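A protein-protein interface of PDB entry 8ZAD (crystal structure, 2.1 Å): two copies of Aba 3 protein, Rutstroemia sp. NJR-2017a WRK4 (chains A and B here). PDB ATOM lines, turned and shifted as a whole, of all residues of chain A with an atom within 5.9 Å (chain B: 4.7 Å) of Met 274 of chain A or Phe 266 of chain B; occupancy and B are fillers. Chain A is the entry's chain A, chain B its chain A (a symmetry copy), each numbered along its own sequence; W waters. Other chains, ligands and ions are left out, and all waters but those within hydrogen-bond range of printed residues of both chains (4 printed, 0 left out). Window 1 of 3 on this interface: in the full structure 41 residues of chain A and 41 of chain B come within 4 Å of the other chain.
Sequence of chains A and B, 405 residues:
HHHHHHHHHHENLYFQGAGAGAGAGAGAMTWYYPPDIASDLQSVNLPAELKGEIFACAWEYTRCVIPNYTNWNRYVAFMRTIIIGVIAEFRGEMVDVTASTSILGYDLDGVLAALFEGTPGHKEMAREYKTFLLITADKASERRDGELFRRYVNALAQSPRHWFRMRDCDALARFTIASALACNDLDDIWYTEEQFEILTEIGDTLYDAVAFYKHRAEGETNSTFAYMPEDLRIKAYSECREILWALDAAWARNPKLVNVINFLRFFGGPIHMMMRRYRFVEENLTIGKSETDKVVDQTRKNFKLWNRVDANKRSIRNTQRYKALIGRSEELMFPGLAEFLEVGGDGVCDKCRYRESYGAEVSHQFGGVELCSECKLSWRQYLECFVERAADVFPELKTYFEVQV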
ATOM      1  N   GLU A  60     -13.007   5.248  23.075  1.00  0.00           N
ATOM      2  CA  GLU A  60     -13.956   5.825  22.075  1.00  0.00           C
ATOM      3  C   GLU A  60     -13.349   5.804  20.663  1.00  0.00           C
ATOM      4  O   GLU A  60     -14.040   5.354  19.737  1.00  0.00           O
ATOM      5  CB  GLU A  60     -14.357   7.239  22.497  1.00  0.00           C
ATOM      6  CG  GLU A  60     -15.305   7.235  23.696  1.00  0.00           C
ATOM      7  CD  GLU A  60     -15.923   8.578  24.024  1.00  0.00           C
ATOM      8  OE1 GLU A  60     -16.461   8.689  25.163  1.00  0.00           O
ATOM      9  OE2 GLU A  60     -15.890   9.502  23.140  1.00  0.00           O
ATOM     10  N   ARG A  63     -13.089   2.152  19.450  1.00  0.00           N
ATOM     11  CA  ARG A  63     -14.406   1.566  19.106  1.00  0.00           C
ATOM     12  C   ARG A  63     -14.954   2.173  17.793  1.00  0.00           C
ATOM     13  O   ARG A  63     -15.705   1.469  17.097  1.00  0.00           O
ATOM     14  CB  ARG A  63     -15.398   1.785  20.247  1.00  0.00           C
ATOM     15  CG  ARG A  63     -15.083   1.016  21.532  1.00  0.00           C
ATOM     16  CD  ARG A  63     -15.245  -0.463  21.344  1.00  0.00           C
ATOM     17  NE  ARG A  63     -16.653  -0.693  21.097  1.00  0.00           N
ATOM     18  CZ  ARG A  63     -17.153  -1.225  20.007  1.00  0.00           C
ATOM     19  NH1 ARG A  63     -16.353  -1.628  19.032  1.00  0.00           N
ATOM     20  NH2 ARG A  63     -18.459  -1.315  19.878  1.00  0.00           N
ATOM     21  N   CYS A  64     -14.645   3.435  17.487  1.00  0.00           N
ATOM     22  CA  CYS A  64     -15.188   4.155  16.318  1.00  0.00           C
ATOM     23  C   CYS A  64     -14.477   3.689  15.045  1.00  0.00           C
ATOM     24  O   CYS A  64     -15.162   3.453  14.050  1.00  0.00           O
ATOM     25  CB  CYS A  64     -15.079   5.667  16.476  1.00  0.00           C
ATOM     26  SG  CYS A  64     -16.281   6.387  17.626  1.00  0.00           S
ATOM     27  N   PRO A  67     -14.406  -0.868  14.758  1.00  0.00           N
ATOM     28  CA  PRO A  67     -15.640  -1.196  15.465  1.00  0.00           C
ATOM     29  C   PRO A  67     -15.838  -2.701  15.663  1.00  0.00           C
ATOM     30  O   PRO A  67     -16.670  -3.059  16.472  1.00  0.00           O
ATOM     31  CB  PRO A  67     -16.749  -0.633  14.560  1.00  0.00           C
ATOM     32  CG  PRO A  67     -16.015   0.296  13.618  1.00  0.00           C
ATOM     33  CD  PRO A  67     -14.662  -0.361  13.402  1.00  0.00           C
ATOM     34  N   PHE A 266     -15.780   5.328   8.932  1.00  0.00           N
ATOM     35  CA  PHE A 266     -16.124   5.895  10.264  1.00  0.00           C
ATOM     36  C   PHE A 266     -15.140   7.006  10.644  1.00  0.00           C
ATOM     37  O   PHE A 266     -15.577   8.013  11.199  1.00  0.00           O
ATOM     38  CB  PHE A 266     -16.222   4.769  11.284  1.00  0.00           C
ATOM     39  CG  PHE A 266     -17.280   3.778  10.895  1.00  0.00           C
ATOM     40  CD1 PHE A 266     -18.503   4.200  10.375  1.00  0.00           C
ATOM     41  CD2 PHE A 266     -17.047   2.419  10.979  1.00  0.00           C
ATOM     42  CE1 PHE A 266     -19.490   3.282  10.049  1.00  0.00           C
ATOM     43  CE2 PHE A 266     -18.021   1.504  10.591  1.00  0.00           C
ATOM     44  CZ  PHE A 266     -19.240   1.933  10.142  1.00  0.00           C
ATOM     45  N   PHE A 267     -13.862   6.836  10.286  1.00  0.00           N
ATOM     46  CA  PHE A 267     -12.794   7.847  10.424  1.00  0.00           C
ATOM     47  C   PHE A 267     -13.131   9.068   9.571  1.00  0.00           C
ATOM     48  O   PHE A 267     -13.002  10.168  10.123  1.00  0.00           O
ATOM     49  CB  PHE A 267     -11.453   7.235  10.028  1.00  0.00           C
ATOM     50  CG  PHE A 267     -10.301   8.194   9.991  1.00  0.00           C
ATOM     51  CD1 PHE A 267      -9.669   8.579  11.164  1.00  0.00           C
ATOM     52  CD2 PHE A 267      -9.874   8.739   8.787  1.00  0.00           C
ATOM     53  CE1 PHE A 267      -8.595   9.463  11.129  1.00  0.00           C
ATOM     54  CE2 PHE A 267      -8.794   9.607   8.753  1.00  0.00           C
ATOM     55  CZ  PHE A 267      -8.155   9.972   9.924  1.00  0.00           C
ATOM     56  N   PRO A 270     -17.554  10.717  10.214  1.00  0.00           N
ATOM     57  CA  PRO A 270     -18.509  10.266  11.237  1.00  0.00           C
ATOM     58  C   PRO A 270     -18.018  10.331  12.683  1.00  0.00           C
ATOM     59  O   PRO A 270     -18.865  10.540  13.555  1.00  0.00           O
ATOM     60  CB  PRO A 270     -18.795   8.841  10.783  1.00  0.00           C
ATOM     61  CG  PRO A 270     -18.755   8.984   9.277  1.00  0.00           C
ATOM     62  CD  PRO A 270     -17.525   9.834   9.043  1.00  0.00           C
ATOM     63  N   ILE A 271     -16.713  10.194  12.947  1.00  0.00           N
ATOM     64  CA  ILE A 271     -16.223  10.319  14.351  1.00  0.00           C
ATOM     65  C   ILE A 271     -16.630  11.652  14.993  1.00  0.00           C
ATOM     66  O   ILE A 271     -16.707  11.675  16.249  1.00  0.00           O
ATOM     67  CB  ILE A 271     -14.710  10.124  14.506  1.00  0.00           C
ATOM     68  CG1 ILE A 271     -13.912  10.827  13.413  1.00  0.00           C
ATOM     69  CG2 ILE A 271     -14.395   8.646  14.627  1.00  0.00           C
ATOM     70  CD1 ILE A 271     -12.399  10.549  13.506  1.00  0.00           C
ATOM     71  N   HIS A 272     -16.814  12.721  14.226  1.00  0.00           N
ATOM     72  CA  HIS A 272     -17.188  14.064  14.765  1.00  0.00           C
ATOM     73  C   HIS A 272     -18.524  13.928  15.510  1.00  0.00           C
ATOM     74  O   HIS A 272     -18.702  14.580  16.529  1.00  0.00           O
ATOM     75  CB  HIS A 272     -17.213  15.127  13.654  1.00  0.00           C
ATOM     76  CG  HIS A 272     -15.866  15.428  13.071  1.00  0.00           C
ATOM     77  ND1 HIS A 272     -15.178  16.593  13.349  1.00  0.00           N
ATOM     78  CD2 HIS A 272     -15.090  14.747  12.186  1.00  0.00           C
ATOM     79  CE1 HIS A 272     -14.028  16.606  12.701  1.00  0.00           C
ATOM     80  NE2 HIS A 272     -13.960  15.489  11.953  1.00  0.00           N
ATOM     81  N   MET A 273     -19.413  13.042  15.070  1.00  0.00           N
ATOM     82  CA  MET A 273     -20.711  12.840  15.762  1.00  0.00           C
ATOM     83  C   MET A 273     -20.608  11.869  16.958  1.00  0.00           C
ATOM     84  O   MET A 273     -21.447  11.970  17.866  1.00  0.00           O
ATOM     85  CB  MET A 273     -21.746  12.311  14.781  1.00  0.00           C
ATOM     86  CG  MET A 273     -21.946  13.245  13.602  1.00  0.00           C
ATOM     87  SD  MET A 273     -23.288  12.781  12.505  1.00  0.00           S
ATOM     88  CE  MET A 273     -24.539  12.335  13.686  1.00  0.00           C
ATOM     89  N   MET A 274     -19.641  10.964  16.985  1.00  0.00           N
ATOM     90  CA  MET A 274     -19.697   9.772  17.883  1.00  0.00           C
ATOM     91  C   MET A 274     -18.818   9.980  19.120  1.00  0.00           C
ATOM     92  O   MET A 274     -19.150   9.418  20.163  1.00  0.00           O
ATOM     93  CB  MET A 274     -19.251   8.507  17.142  1.00  0.00           C
ATOM     94  CG  MET A 274     -19.983   8.339  15.814  1.00  0.00           C
ATOM     95  SD  MET A 274     -19.566   6.776  14.992  1.00  0.00           S
ATOM     96  CE  MET A 274     -17.929   7.122  14.386  1.00  0.00           C
ATOM     97  N   MET A 275     -17.702  10.686  18.976  1.00  0.00           N
ATOM     98  CA  MET A 275     -16.695  10.819  20.056  1.00  0.00           C
ATOM     99  C   MET A 275     -16.986  12.076  20.862  1.00  0.00           C
ATOM    100  O   MET A 275     -17.141  13.144  20.257  1.00  0.00           O
ATOM    101  CB  MET A 275     -15.282  10.888  19.500  1.00  0.00           C
ATOM    102  CG  MET A 275     -14.804   9.550  19.023  1.00  0.00           C
ATOM    103  SD  MET A 275     -13.124   9.670  18.462  1.00  0.00           S
ATOM    104  CE  MET A 275     -12.371  10.093  20.029  1.00  0.00           C
ATOM    105  N   ARG A 276     -17.046  11.921  22.181  1.00  0.00           N
ATOM    106  CA  ARG A 276     -17.322  13.042  23.108  1.00  0.00           C
ATOM    107  C   ARG A 276     -16.205  14.086  23.012  1.00  0.00           C
ATOM    108  O   ARG A 276     -16.514  15.236  23.296  1.00  0.00           O
ATOM    109  CB  ARG A 276     -17.552  12.499  24.515  1.00  0.00           C
ATOM    110  CG  ARG A 276     -18.741  11.544  24.603  1.00  0.00           C
ATOM    111  CD  ARG A 276     -18.585  10.544  25.748  1.00  0.00           C
ATOM    112  NE  ARG A 276     -18.857  11.183  27.018  1.00  0.00           N
ATOM    113  CZ  ARG A 276     -18.417  10.780  28.203  1.00  0.00           C
ATOM    114  NH1 ARG A 276     -18.753  11.496  29.261  1.00  0.00           N
ATOM    115  NH2 ARG A 276     -17.647   9.702  28.337  1.00  0.00           N
ATOM    116  N   PHE A 280     -19.827  18.178  18.576  1.00  0.00           N
ATOM    117  CA  PHE A 280     -21.163  18.017  17.949  1.00  0.00           C
ATOM    118  C   PHE A 280     -22.266  18.533  18.896  1.00  0.00           C
ATOM    119  O   PHE A 280     -23.132  19.302  18.443  1.00  0.00           O
ATOM    120  CB  PHE A 280     -21.373  16.551  17.554  1.00  0.00           C
ATOM    121  CG  PHE A 280     -22.589  16.321  16.706  1.00  0.00           C
ATOM    122  CD1 PHE A 280     -22.789  17.049  15.542  1.00  0.00           C
ATOM    123  CD2 PHE A 280     -23.538  15.383  17.079  1.00  0.00           C
ATOM    124  CE1 PHE A 280     -23.920  16.845  14.761  1.00  0.00           C
ATOM    125  CE2 PHE A 280     -24.673  15.191  16.307  1.00  0.00           C
ATOM    126  CZ  PHE A 280     -24.856  15.901  15.139  1.00  0.00           C
ATOM    127  N   CYS B  64     -23.898   0.321   6.596  1.00  0.00           N
ATOM    128  CA  CYS B  64     -23.780   1.381   7.616  1.00  0.00           C
ATOM    129  C   CYS B  64     -24.253   0.853   8.972  1.00  0.00           C
ATOM    130  O   CYS B  64     -23.573   1.108   9.965  1.00  0.00           O
ATOM    131  CB  CYS B  64     -24.548   2.639   7.227  1.00  0.00           C
ATOM    132  SG  CYS B  64     -23.753   3.630   5.933  1.00  0.00           S
ATOM    133  N   PRO B  67     -22.288  -3.145   9.975  1.00  0.00           N
ATOM    134  CA  PRO B  67     -21.011  -2.992   9.282  1.00  0.00           C
ATOM    135  C   PRO B  67     -20.154  -4.259   9.316  1.00  0.00           C
ATOM    136  O   PRO B  67     -19.219  -4.329   8.542  1.00  0.00           O
ATOM    137  CB  PRO B  67     -20.307  -1.857  10.045  1.00  0.00           C
ATOM    138  CG  PRO B  67     -21.414  -1.221  10.856  1.00  0.00           C
ATOM    139  CD  PRO B  67     -22.336  -2.371  11.224  1.00  0.00           C
ATOM    140  N   ARG B 241     -26.173   9.200  23.927  1.00  0.00           N
ATOM    141  CA  ARG B 241     -24.818   8.884  23.416  1.00  0.00           C
ATOM    142  C   ARG B 241     -23.933   8.433  24.582  1.00  0.00           C
ATOM    143  O   ARG B 241     -23.150   7.490  24.434  1.00  0.00           O
ATOM    144  CB  ARG B 241     -24.222  10.095  22.713  1.00  0.00           C
ATOM    145  CG  ARG B 241     -22.840   9.799  22.169  1.00  0.00           C
ATOM    146  CD  ARG B 241     -22.384  10.915  21.289  1.00  0.00           C
ATOM    147  NE  ARG B 241     -21.928  12.024  22.122  1.00  0.00           N
ATOM    148  CZ  ARG B 241     -21.361  13.119  21.643  1.00  0.00           C
ATOM    149  NH1 ARG B 241     -21.176  13.250  20.338  1.00  0.00           N
ATOM    150  NH2 ARG B 241     -20.956  14.067  22.473  1.00  0.00           N
ATOM    151  N   TRP B 245     -22.216   4.864  25.287  1.00  0.00           N
ATOM    152  CA  TRP B 245     -20.779   4.638  25.633  1.00  0.00           C
ATOM    153  C   TRP B 245     -20.657   3.803  26.924  1.00  0.00           C
ATOM    154  O   TRP B 245     -19.850   2.851  26.977  1.00  0.00           O
ATOM    155  CB  TRP B 245     -20.064   5.982  25.760  1.00  0.00           C
ATOM    156  CG  TRP B 245     -19.660   6.539  24.440  1.00  0.00           C
ATOM    157  CD1 TRP B 245     -19.963   7.757  23.909  1.00  0.00           C
ATOM    158  CD2 TRP B 245     -18.787   5.891  23.506  1.00  0.00           C
ATOM    159  NE1 TRP B 245     -19.371   7.898  22.686  1.00  0.00           N
ATOM    160  CE2 TRP B 245     -18.660   6.760  22.400  1.00  0.00           C
ATOM    161  CE3 TRP B 245     -18.119   4.662  23.497  1.00  0.00           C
ATOM    162  CZ2 TRP B 245     -17.864   6.444  21.314  1.00  0.00           C
ATOM    163  CZ3 TRP B 245     -17.374   4.332  22.393  1.00  0.00           C
ATOM    164  CH2 TRP B 245     -17.270   5.203  21.311  1.00  0.00           C
ATOM    165  N   ASN B 262     -22.762  -1.142  17.742  1.00  0.00           N
ATOM    166  CA  ASN B 262     -22.364  -0.549  16.443  1.00  0.00           C
ATOM    167  C   ASN B 262     -23.657  -0.114  15.738  1.00  0.00           C
ATOM    168  O   ASN B 262     -23.696   1.002  15.191  1.00  0.00           O
ATOM    169  CB  ASN B 262     -21.473  -1.486  15.607  1.00  0.00           C
ATOM    170  CG  ASN B 262     -20.121  -1.773  16.243  1.00  0.00           C
ATOM    171  OD1 ASN B 262     -19.706  -1.071  17.166  1.00  0.00           O
ATOM    172  ND2 ASN B 262     -19.418  -2.786  15.743  1.00  0.00           N
ATOM    173  N   PHE B 263     -24.698  -0.942  15.769  1.00  0.00           N
ATOM    174  CA  PHE B 263     -25.968  -0.609  15.082  1.00  0.00           C
ATOM    175  C   PHE B 263     -26.437   0.734  15.617  1.00  0.00           C
ATOM    176  O   PHE B 263     -26.650   1.668  14.846  1.00  0.00           O
ATOM    177  CB  PHE B 263     -27.068  -1.648  15.272  1.00  0.00           C
ATOM    178  CG  PHE B 263     -28.424  -1.076  14.958  1.00  0.00           C
ATOM    179  CD1 PHE B 263     -28.731  -0.645  13.670  1.00  0.00           C
ATOM    180  CD2 PHE B 263     -29.359  -0.862  15.956  1.00  0.00           C
ATOM    181  CE1 PHE B 263     -29.951  -0.049  13.389  1.00  0.00           C
ATOM    182  CE2 PHE B 263     -30.571  -0.253  15.669  1.00  0.00           C
ATOM    183  CZ  PHE B 263     -30.869   0.142  14.390  1.00  0.00           C
ATOM    184  N   LEU B 264     -26.599   0.815  16.929  1.00  0.00           N
ATOM    185  CA  LEU B 264     -27.167   2.033  17.556  1.00  0.00           C
ATOM    186  C   LEU B 264     -26.272   3.234  17.246  1.00  0.00           C
ATOM    187  O   LEU B 264     -26.830   4.299  16.967  1.00  0.00           O
ATOM    188  CB  LEU B 264     -27.320   1.790  19.052  1.00  0.00           C
ATOM    189  CG  LEU B 264     -28.348   0.726  19.409  1.00  0.00           C
ATOM    190  CD1 LEU B 264     -28.282   0.417  20.892  1.00  0.00           C
ATOM    191  CD2 LEU B 264     -29.751   1.133  18.947  1.00  0.00           C
ATOM    192  N   ARG B 265     -24.951   3.063  17.305  1.00  0.00           N
ATOM    193  CA  ARG B 265     -23.977   4.181  17.145  1.00  0.00           C
ATOM    194  C   ARG B 265     -24.026   4.714  15.707  1.00  0.00           C
ATOM    195  O   ARG B 265     -24.075   5.939  15.527  1.00  0.00           O
ATOM    196  CB  ARG B 265     -22.569   3.727  17.537  1.00  0.00           C
ATOM    197  CG  ARG B 265     -21.467   4.743  17.260  1.00  0.00           C
ATOM    198  CD  ARG B 265     -20.172   4.445  18.005  1.00  0.00           C
ATOM    199  NE  ARG B 265     -20.399   4.455  19.441  1.00  0.00           N
ATOM    200  CZ  ARG B 265     -20.043   3.519  20.320  1.00  0.00           C
ATOM    201  NH1 ARG B 265     -20.369   3.685  21.583  1.00  0.00           N
ATOM    202  NH2 ARG B 265     -19.363   2.444  19.974  1.00  0.00           N
ATOM    203  N   PHE B 266     -24.052   3.840  14.698  1.00  0.00           N
ATOM    204  CA  PHE B 266     -23.949   4.284  13.281  1.00  0.00           C
ATOM    205  C   PHE B 266     -25.311   4.761  12.769  1.00  0.00           C
ATOM    206  O   PHE B 266     -25.351   5.757  12.046  1.00  0.00           O
ATOM    207  CB  PHE B 266     -23.319   3.176  12.449  1.00  0.00           C
ATOM    208  CG  PHE B 266     -21.944   2.839  12.948  1.00  0.00           C
ATOM    209  CD1 PHE B 266     -21.061   3.840  13.350  1.00  0.00           C
ATOM    210  CD2 PHE B 266     -21.541   1.525  13.088  1.00  0.00           C
ATOM    211  CE1 PHE B 266     -19.779   3.525  13.779  1.00  0.00           C
ATOM    212  CE2 PHE B 266     -20.275   1.217  13.578  1.00  0.00           C
ATOM    213  CZ  PHE B 266     -19.395   2.211  13.908  1.00  0.00           C
ATOM    214  N   PHE B 267     -26.390   4.096  13.197  1.00  0.00           N
ATOM    215  CA  PHE B 267     -27.792   4.486  12.941  1.00  0.00           C
ATOM    216  C   PHE B 267     -28.069   5.846  13.578  1.00  0.00           C
ATOM    217  O   PHE B 267     -28.656   6.670  12.866  1.00  0.00           O
ATOM    218  CB  PHE B 267     -28.731   3.409  13.479  1.00  0.00           C
ATOM    219  CG  PHE B 267     -30.191   3.743  13.408  1.00  0.00           C
ATOM    220  CD1 PHE B 267     -30.884   3.615  12.213  1.00  0.00           C
ATOM    221  CD2 PHE B 267     -30.861   4.221  14.526  1.00  0.00           C
ATOM    222  CE1 PHE B 267     -32.240   3.917  12.149  1.00  0.00           C
ATOM    223  CE2 PHE B 267     -32.216   4.506  14.464  1.00  0.00           C
ATOM    224  CZ  PHE B 267     -32.906   4.358  13.274  1.00  0.00           C
ATOM    225  N   GLY B 268     -27.591   6.071  14.819  1.00  0.00           N
ATOM    226  CA  GLY B 268     -27.904   7.239  15.677  1.00  0.00           C
ATOM    227  C   GLY B 268     -27.313   8.561  15.195  1.00  0.00           C
ATOM    228  O   GLY B 268     -26.726   9.293  16.018  1.00  0.00           O
ATOM    229  N   GLY B 269     -27.467   8.883  13.913  1.00  0.00           N
ATOM    230  CA  GLY B 269     -26.987  10.133  13.313  1.00  0.00           C
ATOM    231  C   GLY B 269     -25.913   9.934  12.250  1.00  0.00           C
ATOM    232  O   GLY B 269     -25.966  10.538  11.186  1.00  0.00           O
ATOM    233  N   PRO B 270     -24.833   9.177  12.519  1.00  0.00           N
ATOM    234  CA  PRO B 270     -23.739   9.046  11.545  1.00  0.00           C
ATOM    235  C   PRO B 270     -24.152   8.656  10.127  1.00  0.00           C
ATOM    236  O   PRO B 270     -23.457   9.082   9.201  1.00  0.00           O
ATOM    237  CB  PRO B 270     -22.862   7.991  12.207  1.00  0.00           C
ATOM    238  CG  PRO B 270     -23.019   8.336  13.672  1.00  0.00           C
ATOM    239  CD  PRO B 270     -24.507   8.571  13.815  1.00  0.00           C
ATOM    240  N   ILE B 271     -25.247   7.910   9.936  1.00  0.00           N
ATOM    241  CA  ILE B 271     -25.688   7.580   8.549  1.00  0.00           C
ATOM    242  C   ILE B 271     -25.898   8.834   7.691  1.00  0.00           C
ATOM    243  O   ILE B 271     -25.792   8.692   6.445  1.00  0.00           O
ATOM    244  CB  ILE B 271     -26.947   6.706   8.484  1.00  0.00           C
ATOM    245  CG1 ILE B 271     -28.015   7.140   9.482  1.00  0.00           C
ATOM    246  CG2 ILE B 271     -26.562   5.245   8.608  1.00  0.00           C
ATOM    247  CD1 ILE B 271     -29.239   6.203   9.490  1.00  0.00           C
ATOM    248  N   MET B 274     -22.825   9.264   5.720  1.00  0.00           N
ATOM    249  CA  MET B 274     -22.208   8.098   5.020  1.00  0.00           C
ATOM    250  C   MET B 274     -23.040   7.694   3.799  1.00  0.00           C
ATOM    251  O   MET B 274     -22.452   7.183   2.846  1.00  0.00           O
ATOM    252  CB  MET B 274     -22.067   6.902   5.966  1.00  0.00           C
ATOM    253  CG  MET B 274     -21.388   7.291   7.276  1.00  0.00           C
ATOM    254  SD  MET B 274     -21.092   5.857   8.348  1.00  0.00           S
ATOM    255  CE  MET B 274     -22.731   5.524   8.953  1.00  0.00           C
HETATM  256  O   HOH W   1     -18.351   1.520  17.367  1.00  0.00           O
HETATM  257  O   HOH W   2     -19.027  14.972  19.178  1.00  0.00           O
HETATM  258  O   HOH W   3     -20.013  16.568  21.520  1.00  0.00           O
HETATM  259  O   HOH W   4     -21.135   7.443  19.915  1.00  0.00           O
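NH2 of Arg 63 of chain A sits at hydrogen-bond distance from OD1 of Asn 262 of chain B, 3.0 Å away. ND2 of Asn 262 of chain B lies within hydrogen-bond range of O of Pro 67 of chain A. The backbone carbonyl oxygen (O) of Met 273 of chain A lies within hydrogen-bond range of the guanidinium group (NH1) of Arg 241 of chain B (2.8 Å). The indole nitrogen of Trp 245 of chain B is in hydrogen-bond range of the backbone carbonyl oxygen of Met 274 of chain A, 3.0 Å away. SD of Met 273 of chain A lies close to O of Gly 269 of chain B, 3.7 Å away.
Of chain B, only Arg 241, Trp 245, Arg 265, Phe 266 and Pro 270 come within 4 Å of Met 274 of chain A. Phe 266 of chain B touches just these residues of chain A: Pro 67, Phe 266 and Met 274. Of the printed residues of chain B, Arg 63 of chain A touches Trp 245 (3.9 Å), Asn 262 (3.0 Å) and Arg 265 (3.9 Å). Printed residues of chain A within 4 Å of Pro 67 of chain B: Phe 266 (3.9 Å). Printed residues of chain A within 4 Å of Met 274 of chain B: Phe 266 and Pro 270. Of the printed residues of chain B, Glu 60 of chain A touches Trp 245. The nearest residue of chain A that does not touch Phe 266 of chain B is Cys 64 of chain A (4.4 Å).
Cys 64 of chain A touches Trp 245 of chain B. Phe 266 of chain B touches Pro 67 of chain A. CE2 of Phe 266 of chain B touches CZ of Phe 266 of chain A, at 3.7 Å. Pro 270 of chain A touches Met 274 of chain B. CE of Met 273 of chain A touches N of Pro 270 of chain B (3.4 Å). CD of Arg 241 of chain B touches O of Met 274 of chain A, at 3.7 Å. Met 274 of chain A touches Phe 266 of chain B. Pro 270 of chain B touches Met 274 of chain A (CG to CG, 3.7 Å). Arg 276 of chain A touches Arg 241 of chain B. Arg 276 of chain A touches Trp 245 of chain B (CD to CD1, 3.6 Å).
SG of Cys 64 of chain A lies within hydrogen-bond range of O of Glu 60 of chain A (3.2 Å). The side-chain carboxylate (OE1) of Glu 60 of chain A is in salt-bridge range of the guanidinium group (NH2) of Arg 276 of chain A (3.5 Å). The guanidinium group (NH1) of Arg 63 of chain A lies within hydrogen-bond range of the backbone carbonyl oxygen (O) of Pro 67 of chain A, 2.9 Å away. The backbone carbonyl oxygen (O) of Phe 266 of chain A lies within hydrogen-bond range of the backbone NH (N) of Ile 271 of chain A (3.0 Å). O of Phe 266 of chain B is in hydrogen-bond range of N of Ile 271 of chain B (3.0 Å).
Printed residues of chain B that touch a printed residue of chain A: Pro 67, Arg 241, Trp 245, Asn 262, Arg 265, Phe 266, Gly 269, Pro 270 and Met 274. Hydrophobic or aromatic side chains of chain B that line the printed part of chain A: Pro 67, Trp 245, Phe 266, Pro 270 and Met 274. Hydrophobic or aromatic side chains of chain A within 4 Å of the printed part of chain B: Pro 67, Phe 266, Pro 270, Met 273 and Met 274. Among the printed residues, no Asp or Glu carboxylate lies within 4 Å of a Lys or Arg side-chain nitrogen of the other chain.
Pro 67 of chain A touches Phe 266 of chain B, and with the chains exchanged Phe 266 of chain A touches Pro 67 of chain B. Phe 266 of chain B touches its own counterpart, Phe 266 of chain A. Phe 266 of chain A touches Met 274 of chain B, and with the chains exchanged Met 274 of chain A touches Phe 266 of chain B. Pro 270 of chain A touches Met 274 of chain B, and with the chains exchanged Met 274 of chain A touches Pro 270 of chain B.
Water W1 lies within hydrogen-bond range of O of Arg 63 of chain A (2.7 Å), OD1 of Asn 262 of chain B (2.9 Å) and NH2 of Arg 265 of chain B (2.9 Å). Water W2 lies within hydrogen-bond range of the backbone carbonyl oxygen (O) of His 272 of chain A, the backbone carbonyl oxygen (O) of Met 275 of chain A, the guanidinium group (NH1) of Arg 241 of chain B and the backbone NH (N) of Phe 280 of chain A. Water W4 lies within hydrogen-bond range of O of Met 274 of chain A (2.8 Å), NE of Arg 265 of chain B (3.1 Å) and NE1 of Trp 245 of chain B (3.3 Å). Water W3 lies within hydrogen-bond range of the guanidinium group of Arg 241 of chain B (2.8 Å) and the backbone NH of Phe 280 of chain A (3.4 Å).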
